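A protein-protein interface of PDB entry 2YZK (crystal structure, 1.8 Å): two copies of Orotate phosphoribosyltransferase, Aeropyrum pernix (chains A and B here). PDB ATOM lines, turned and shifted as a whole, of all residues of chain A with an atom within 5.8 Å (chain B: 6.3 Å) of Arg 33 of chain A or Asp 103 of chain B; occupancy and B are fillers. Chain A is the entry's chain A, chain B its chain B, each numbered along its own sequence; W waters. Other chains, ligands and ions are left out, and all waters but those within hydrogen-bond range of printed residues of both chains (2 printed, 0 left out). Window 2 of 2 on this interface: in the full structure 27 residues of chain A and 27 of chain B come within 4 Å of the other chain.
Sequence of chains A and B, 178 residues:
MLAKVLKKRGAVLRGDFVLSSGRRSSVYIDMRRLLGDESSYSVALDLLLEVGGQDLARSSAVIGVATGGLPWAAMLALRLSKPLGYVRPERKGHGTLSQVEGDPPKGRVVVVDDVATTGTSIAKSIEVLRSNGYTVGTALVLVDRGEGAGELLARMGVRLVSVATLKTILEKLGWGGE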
ATOM      1  N   ARG A   9      15.948  -6.355   6.156  1.00  0.00           N
ATOM      2  CA  ARG A   9      16.385  -7.444   5.287  1.00  0.00           C
ATOM      3  C   ARG A   9      15.551  -8.718   5.397  1.00  0.00           C
ATOM      4  O   ARG A   9      15.838  -9.706   4.726  1.00  0.00           O
ATOM      5  CB  ARG A   9      17.851  -7.780   5.578  1.00  0.00           C
ATOM      6  CG  ARG A   9      18.833  -6.664   5.238  1.00  0.00           C
ATOM      7  CD  ARG A   9      18.876  -6.433   3.735  1.00  0.00           C
ATOM      8  NE  ARG A   9      19.287  -7.648   3.039  1.00  0.00           N
ATOM      9  CZ  ARG A   9      19.185  -7.839   1.726  1.00  0.00           C
ATOM     10  NH1 ARG A   9      18.686  -6.890   0.943  1.00  0.00           N
ATOM     11  NH2 ARG A   9      19.573  -8.992   1.199  1.00  0.00           N
ATOM     12  N   GLY A  10      14.524  -8.704   6.237  1.00  0.00           N
ATOM     13  CA  GLY A  10      13.707  -9.895   6.391  1.00  0.00           C
ATOM     14  C   GLY A  10      14.438 -10.983   7.158  1.00  0.00           C
ATOM     15  O   GLY A  10      14.095 -12.165   7.059  1.00  0.00           O
ATOM     16  N   ALA A  11      15.454 -10.590   7.919  1.00  0.00           N
ATOM     17  CA  ALA A  11      16.232 -11.539   8.710  1.00  0.00           C
ATOM     18  C   ALA A  11      15.404 -12.001   9.909  1.00  0.00           C
ATOM     19  O   ALA A  11      15.774 -12.930  10.625  1.00  0.00           O
ATOM     20  CB  ALA A  11      17.539 -10.895   9.171  1.00  0.00           C
ATOM     21  N   ASP A  30      16.893 -15.538  10.146  1.00  0.00           N
ATOM     22  CA  ASP A  30      17.836 -15.892   9.093  1.00  0.00           C
ATOM     23  C   ASP A  30      18.851 -14.773   8.897  1.00  0.00           C
ATOM     24  O   ASP A  30      18.635 -13.843   8.119  1.00  0.00           O
ATOM     25  CB  ASP A  30      17.112 -16.167   7.775  1.00  0.00           C
ATOM     26  CG  ASP A  30      18.028 -16.783   6.734  1.00  0.00           C
ATOM     27  OD1 ASP A  30      19.234 -16.932   7.032  1.00  0.00           O
ATOM     28  OD2 ASP A  30      17.550 -17.115   5.626  1.00  0.00           O
ATOM     29  N   MET A  31      19.964 -14.884   9.611  1.00  0.00           N
ATOM     30  CA  MET A  31      21.026 -13.891   9.558  1.00  0.00           C
ATOM     31  C   MET A  31      21.702 -13.840   8.188  1.00  0.00           C
ATOM     32  O   MET A  31      22.372 -12.864   7.850  1.00  0.00           O
ATOM     33  CB  MET A  31      22.059 -14.206  10.640  1.00  0.00           C
ATOM     34  CG  MET A  31      22.392 -13.055  11.573  1.00  0.00           C
ATOM     35  SD  MET A  31      20.976 -12.198  12.332  1.00  0.00           S
ATOM     36  CE  MET A  31      19.788 -13.520  12.635  1.00  0.00           C
ATOM     37  N   ARG A  32      21.527 -14.896   7.401  1.00  0.00           N
ATOM     38  CA  ARG A  32      22.136 -14.945   6.077  1.00  0.00           C
ATOM     39  C   ARG A  32      21.617 -13.819   5.188  1.00  0.00           C
ATOM     40  O   ARG A  32      22.319 -13.352   4.292  1.00  0.00           O
ATOM     41  CB  ARG A  32      21.858 -16.300   5.418  1.00  0.00           C
ATOM     42  CG  ARG A  32      22.511 -17.484   6.129  1.00  0.00           C
ATOM     43  CD  ARG A  32      22.048 -18.809   5.537  1.00  0.00           C
ATOM     44  NE  ARG A  32      20.595 -18.940   5.588  1.00  0.00           N
ATOM     45  CZ  ARG A  32      19.919 -19.998   5.149  1.00  0.00           C
ATOM     46  NH1 ARG A  32      20.561 -21.033   4.624  1.00  0.00           N
ATOM     47  NH2 ARG A  32      18.595 -20.014   5.227  1.00  0.00           N
ATOM     48  N   ARG A  33      20.392 -13.374   5.438  1.00  0.00           N
ATOM     49  CA  ARG A  33      19.815 -12.313   4.625  1.00  0.00           C
ATOM     50  C   ARG A  33      20.529 -10.971   4.758  1.00  0.00           C
ATOM     51  O   ARG A  33      20.343 -10.083   3.935  1.00  0.00           O
ATOM     52  CB  ARG A  33      18.326 -12.170   4.935  1.00  0.00           C
ATOM     53  CG  ARG A  33      17.529 -13.410   4.555  1.00  0.00           C
ATOM     54  CD  ARG A  33      16.059 -13.229   4.858  1.00  0.00           C
ATOM     55  NE  ARG A  33      15.393 -12.323   3.927  1.00  0.00           N
ATOM     56  CZ  ARG A  33      14.973 -12.673   2.713  1.00  0.00           C
ATOM     57  NH1 ARG A  33      15.152 -13.913   2.273  1.00  0.00           N
ATOM     58  NH2 ARG A  33      14.356 -11.787   1.941  1.00  0.00           N
ATOM     59  N   LEU A  34      21.361 -10.821   5.780  1.00  0.00           N
ATOM     60  CA  LEU A  34      22.095  -9.573   5.943  1.00  0.00           C
ATOM     61  C   LEU A  34      23.243  -9.491   4.936  1.00  0.00           C
ATOM     62  O   LEU A  34      23.723  -8.405   4.611  1.00  0.00           O
ATOM     63  CB  LEU A  34      22.674  -9.470   7.351  1.00  0.00           C
ATOM     64  CG  LEU A  34      21.686  -9.524   8.513  1.00  0.00           C
ATOM     65  CD1 LEU A  34      22.452  -9.294   9.803  1.00  0.00           C
ATOM     66  CD2 LEU A  34      20.612  -8.457   8.344  1.00  0.00           C
ATOM     67  N   LEU A  35      23.680 -10.647   4.448  1.00  0.00           N
ATOM     68  CA  LEU A  35      24.805 -10.700   3.514  1.00  0.00           C
ATOM     69  C   LEU A  35      24.534 -10.084   2.149  1.00  0.00           C
ATOM     70  O   LEU A  35      25.453  -9.600   1.489  1.00  0.00           O
ATOM     71  CB  LEU A  35      25.258 -12.154   3.334  1.00  0.00           C
ATOM     72  CG  LEU A  35      25.746 -12.834   4.615  1.00  0.00           C
ATOM     73  CD1 LEU A  35      25.924 -14.324   4.374  1.00  0.00           C
ATOM     74  CD2 LEU A  35      27.058 -12.195   5.059  1.00  0.00           C
ATOM     75  N   GLY A  36      23.272 -10.087   1.735  1.00  0.00           N
ATOM     76  CA  GLY A  36      22.929  -9.542   0.432  1.00  0.00           C
ATOM     77  C   GLY A  36      22.815  -8.027   0.352  1.00  0.00           C
ATOM     78  O   GLY A  36      22.265  -7.505  -0.613  1.00  0.00           O
ATOM     79  N   ASP A  37      23.326  -7.322   1.356  1.00  0.00           N
ATOM     80  CA  ASP A  37      23.280  -5.858   1.367  1.00  0.00           C
ATOM     81  C   ASP A  37      24.500  -5.342   2.127  1.00  0.00           C
ATOM     82  O   ASP A  37      24.610  -5.545   3.334  1.00  0.00           O
ATOM     83  CB  ASP A  37      21.992  -5.381   2.047  1.00  0.00           C
ATOM     84  CG  ASP A  37      21.797  -3.881   1.945  1.00  0.00           C
ATOM     85  OD1 ASP A  37      21.697  -3.362   0.808  1.00  0.00           O
ATOM     86  OD2 ASP A  37      21.745  -3.219   3.002  1.00  0.00           O
ATOM     87  N   SER A  40      23.882  -3.542   5.336  1.00  0.00           N
ATOM     88  CA  SER A  40      23.500  -4.419   6.429  1.00  0.00           C
ATOM     89  C   SER A  40      24.640  -5.251   6.994  1.00  0.00           C
ATOM     90  O   SER A  40      24.828  -5.294   8.213  1.00  0.00           O
ATOM     91  CB  SER A  40      22.358  -5.332   5.976  1.00  0.00           C
ATOM     92  OG  SER A  40      21.243  -4.550   5.573  1.00  0.00           O
ATOM     93  N   LEU B  84      26.660 -10.008  -1.049  1.00  0.00           N
ATOM     94  CA  LEU B  84      27.120 -11.388  -1.122  1.00  0.00           C
ATOM     95  C   LEU B  84      25.922 -12.315  -1.142  1.00  0.00           C
ATOM     96  O   LEU B  84      24.892 -12.024  -0.541  1.00  0.00           O
ATOM     97  CB  LEU B  84      27.961 -11.747   0.105  1.00  0.00           C
ATOM     98  CG  LEU B  84      28.338 -13.229   0.215  1.00  0.00           C
ATOM     99  CD1 LEU B  84      29.381 -13.572  -0.846  1.00  0.00           C
ATOM    100  CD2 LEU B  84      28.878 -13.521   1.602  1.00  0.00           C
ATOM    101  N   GLY B  85      26.069 -13.433  -1.834  1.00  0.00           N
ATOM    102  CA  GLY B  85      25.018 -14.426  -1.884  1.00  0.00           C
ATOM    103  C   GLY B  85      25.730 -15.751  -2.054  1.00  0.00           C
ATOM    104  O   GLY B  85      26.924 -15.773  -2.351  1.00  0.00           O
ATOM    105  N   GLN B  99      17.231 -21.782  -2.951  1.00  0.00           N
ATOM    106  CA  GLN B  99      17.255 -20.326  -2.927  1.00  0.00           C
ATOM    107  C   GLN B  99      18.695 -19.831  -2.929  1.00  0.00           C
ATOM    108  O   GLN B  99      19.633 -20.602  -2.723  1.00  0.00           O
ATOM    109  CB  GLN B  99      16.536 -19.809  -1.674  1.00  0.00           C
ATOM    110  CG  GLN B  99      17.254 -20.135  -0.367  1.00  0.00           C
ATOM    111  CD  GLN B  99      16.421 -19.823   0.867  1.00  0.00           C
ATOM    112  OE1 GLN B  99      16.909 -19.896   1.997  1.00  0.00           O
ATOM    113  NE2 GLN B  99      15.155 -19.482   0.656  1.00  0.00           N
ATOM    114  N   VAL B 100      18.867 -18.545  -3.196  1.00  0.00           N
ATOM    115  CA  VAL B 100      20.193 -17.952  -3.176  1.00  0.00           C
ATOM    116  C   VAL B 100      20.302 -17.343  -1.783  1.00  0.00           C
ATOM    117  O   VAL B 100      19.650 -16.345  -1.477  1.00  0.00           O
ATOM    118  CB  VAL B 100      20.334 -16.856  -4.253  1.00  0.00           C
ATOM    119  CG1 VAL B 100      21.731 -16.269  -4.219  1.00  0.00           C
ATOM    120  CG2 VAL B 100      20.035 -17.446  -5.636  1.00  0.00           C
ATOM    121  N   GLU B 101      21.096 -17.968  -0.920  1.00  0.00           N
ATOM    122  CA  GLU B 101      21.243 -17.473   0.444  1.00  0.00           C
ATOM    123  C   GLU B 101      21.794 -16.048   0.438  1.00  0.00           C
ATOM    124  O   GLU B 101      22.692 -15.732  -0.334  1.00  0.00           O
ATOM    125  CB  GLU B 101      22.174 -18.388   1.243  1.00  0.00           C
ATOM    126  CG  GLU B 101      21.845 -19.880   1.152  1.00  0.00           C
ATOM    127  CD  GLU B 101      20.379 -20.203   1.397  1.00  0.00           C
ATOM    128  OE1 GLU B 101      19.659 -19.364   1.978  1.00  0.00           O
ATOM    129  OE2 GLU B 101      19.950 -21.317   1.015  1.00  0.00           O
ATOM    130  N   GLY B 102      21.243 -15.190   1.294  1.00  0.00           N
ATOM    131  CA  GLY B 102      21.700 -13.810   1.345  1.00  0.00           C
ATOM    132  C   GLY B 102      20.724 -12.864   0.668  1.00  0.00           C
ATOM    133  O   GLY B 102      20.659 -11.683   0.994  1.00  0.00           O
ATOM    134  N   ASP B 103      19.956 -13.400  -0.278  1.00  0.00           N
ATOM    135  CA  ASP B 103      18.975 -12.622  -1.029  1.00  0.00           C
ATOM    136  C   ASP B 103      19.545 -11.321  -1.595  1.00  0.00           C
ATOM    137  O   ASP B 103      19.004 -10.234  -1.374  1.00  0.00           O
ATOM    138  CB  ASP B 103      17.750 -12.329  -0.152  1.00  0.00           C
ATOM    139  CG  ASP B 103      16.616 -11.690  -0.933  1.00  0.00           C
ATOM    140  OD1 ASP B 103      16.387 -12.107  -2.088  1.00  0.00           O
ATOM    141  OD2 ASP B 103      15.945 -10.784  -0.391  1.00  0.00           O
ATOM    142  N   PRO B 104      20.658 -11.414  -2.336  1.00  0.00           N
ATOM    143  CA  PRO B 104      21.246 -10.201  -2.910  1.00  0.00           C
ATOM    144  C   PRO B 104      20.327  -9.622  -3.996  1.00  0.00           C
ATOM    145  O   PRO B 104      19.457 -10.316  -4.522  1.00  0.00           O
ATOM    146  CB  PRO B 104      22.590 -10.693  -3.446  1.00  0.00           C
ATOM    147  CG  PRO B 104      22.303 -12.121  -3.823  1.00  0.00           C
ATOM    148  CD  PRO B 104      21.454 -12.612  -2.672  1.00  0.00           C
ATOM    149  N   PRO B 105      20.510  -8.341  -4.343  1.00  0.00           N
ATOM    150  CA  PRO B 105      19.670  -7.710  -5.367  1.00  0.00           C
ATOM    151  C   PRO B 105      19.732  -8.396  -6.728  1.00  0.00           C
ATOM    152  O   PRO B 105      20.788  -8.859  -7.152  1.00  0.00           O
ATOM    153  CB  PRO B 105      20.184  -6.266  -5.398  1.00  0.00           C
ATOM    154  CG  PRO B 105      21.606  -6.390  -4.952  1.00  0.00           C
ATOM    155  CD  PRO B 105      21.537  -7.412  -3.846  1.00  0.00           C
ATOM    156  N   LYS B 106      18.586  -8.470  -7.401  1.00  0.00           N
ATOM    157  CA  LYS B 106      18.523  -9.106  -8.713  1.00  0.00           C
ATOM    158  C   LYS B 106      19.366  -8.344  -9.732  1.00  0.00           C
ATOM    159  O   LYS B 106      19.410  -7.114  -9.734  1.00  0.00           O
ATOM    160  CB  LYS B 106      17.068  -9.200  -9.198  1.00  0.00           C
ATOM    161  CG  LYS B 106      16.166 -10.078  -8.323  1.00  0.00           C
ATOM    162  CD  LYS B 106      16.682 -11.517  -8.239  1.00  0.00           C
ATOM    163  CE  LYS B 106      15.926 -12.344  -7.199  1.00  0.00           C
ATOM    164  NZ  LYS B 106      14.512 -12.615  -7.602  1.00  0.00           N
ATOM    165  N   TYR B 134      18.263 -14.150 -11.383  1.00  0.00           N
ATOM    166  CA  TYR B 134      19.570 -13.536 -11.565  1.00  0.00           C
ATOM    167  C   TYR B 134      20.121 -13.967 -12.913  1.00  0.00           C
ATOM    168  O   TYR B 134      19.684 -14.964 -13.476  1.00  0.00           O
ATOM    169  CB  TYR B 134      20.551 -14.015 -10.491  1.00  0.00           C
ATOM    170  CG  TYR B 134      20.160 -13.682  -9.073  1.00  0.00           C
ATOM    171  CD1 TYR B 134      20.566 -12.486  -8.476  1.00  0.00           C
ATOM    172  CD2 TYR B 134      19.397 -14.572  -8.316  1.00  0.00           C
ATOM    173  CE1 TYR B 134      20.229 -12.191  -7.161  1.00  0.00           C
ATOM    174  CE2 TYR B 134      19.051 -14.284  -6.999  1.00  0.00           C
ATOM    175  CZ  TYR B 134      19.473 -13.096  -6.429  1.00  0.00           C
ATOM    176  OH  TYR B 134      19.164 -12.822  -5.120  1.00  0.00           O
HETATM  177  O   HOH W   1      19.159 -16.702   2.957  1.00  0.00           O
HETATM  178  O   HOH W   2      18.126  -7.724  -1.950  1.00  0.00           O
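Asp 103 of chain B touches just these residues of chain A: Arg 9 (2.9 Å) and Arg 33 (3.0 Å). Of the printed residues of chain A, Gln 99 of chain B touches Arg 32. Printed residues of chain B within 4 Å of Arg 32 of chain A: Gln 99, Glu 101 and Gly 102. Of the printed residues of chain A, Pro 104 of chain B touches Gly 36. Of the printed residues of chain B, Gly 36 of chain A touches Leu 84, Gly 102, Pro 104 and Pro 105. Of the printed residues of chain A, Glu 101 of chain B touches Arg 32 (3.2 Å). Ala 11 of chain A touches none of the printed residues of chain B. The nearest residue of chain B that does not touch Arg 33 of chain A is Gln 99 of chain B (5.8 Å).
Of the 12 printed residues of chain A, 5 touch a printed residue of chain B. Printed residues of chain A that touch a printed residue of chain B: Arg 9, Arg 32, Arg 33, Leu 35 and Gly 36. Hydrophobic or aromatic side chains of chain A that line the printed part of chain B: Leu 35. Printed residues of chain B that touch a printed residue of chain A: Leu 84, Gln 99, Glu 101, Gly 102, Asp 103, Pro 104 and Pro 105. Hydrophobic or aromatic side chains of chain B that line the printed part of chain A: Leu 84 and Pro 105. Among the printed residues, 12 pairs touch across the chains.
O of Arg 9 of chain A lies within hydrogen-bond range of NE of Arg 33 of chain A, at 2.8 Å. The backbone carbonyl oxygen (O) of Gly 10 of chain A lies close to the guanidinium group (NE) of Arg 33 of chain A, at 3.4 Å. The side-chain carboxylate (OD1) of Asp 30 of chain A lies within salt-bridge range of the guanidinium group (NE) of Arg 32 of chain A. The side-chain amide oxygen (OE1) of Gln 99 of chain B sits close to the side-chain carboxylate (OE1) of Glu 101 of chain B. The side-chain hydroxyl (OH) of Tyr 134 of chain B sits at hydrogen-bond distance from the backbone carbonyl oxygen (O) of Pro 104 of chain B (2.6 Å).
Water W2 lies within hydrogen-bond range of the backbone carbonyl oxygen of Asp 103 of chain B (2.7 Å) and the guanidinium group of Arg 9 of chain A (3.1 Å). Water W1 lies within hydrogen-bond range of OE1 of Glu 101 of chain B, N of Gly 102 of chain B and OD2 of Asp 30 of chain A.
NH2 of Arg 9 of chain A lies within hydrogen-bond range of O of Gly 102 of chain B, 2.9 Å away. NH2 of Arg 9 of chain A lies within hydrogen-bond range of O of Asp 103 of chain B (2.9 Å). The side-chain carboxylate of Glu 101 of chain B lies within salt-bridge range of the guanidinium group of Arg 32 of chain A (3.3 Å). NH2 of Arg 33 of chain A is in salt-bridge range of OD2 of Asp 103 of chain B. The backbone NH (N) of Leu 84 of chain B lies within hydrogen-bond range of the backbone carbonyl oxygen (O) of Leu 35 of chain A, at 2.8 Å. The backbone carbonyl oxygen (O) of Leu 84 of chain B sits close to the backbone NH (N) of Gly 36 of chain A (3.4 Å). The backbone NH (N) of Gly 36 of chain A sits at hydrogen-bond distance from the backbone carbonyl oxygen (O) of Gly 102 of chain B, 3.2 Å away. The backbone carbonyl oxygen (O) of Arg 33 of chain A sits close to the backbone carbonyl oxygen (O) of Gly 102 of chain B (3.4 Å).
OE1 of Gln 99 of chain B touches NH2 of Arg 32 of chain A, at 3.6 Å. Gly 102 of chain B touches Arg 32 of chain A. Gly 36 of chain A touches Pro 104 of chain B (O to CA, 3.7 Å). CD of Pro 105 of chain B touches O of Gly 36 of chain A, 3.3 Å away.
No position is printed for both chains. Of the 12 pairs that touch across the chains among the printed residues, none has its exchanged pair printed and touching as well.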
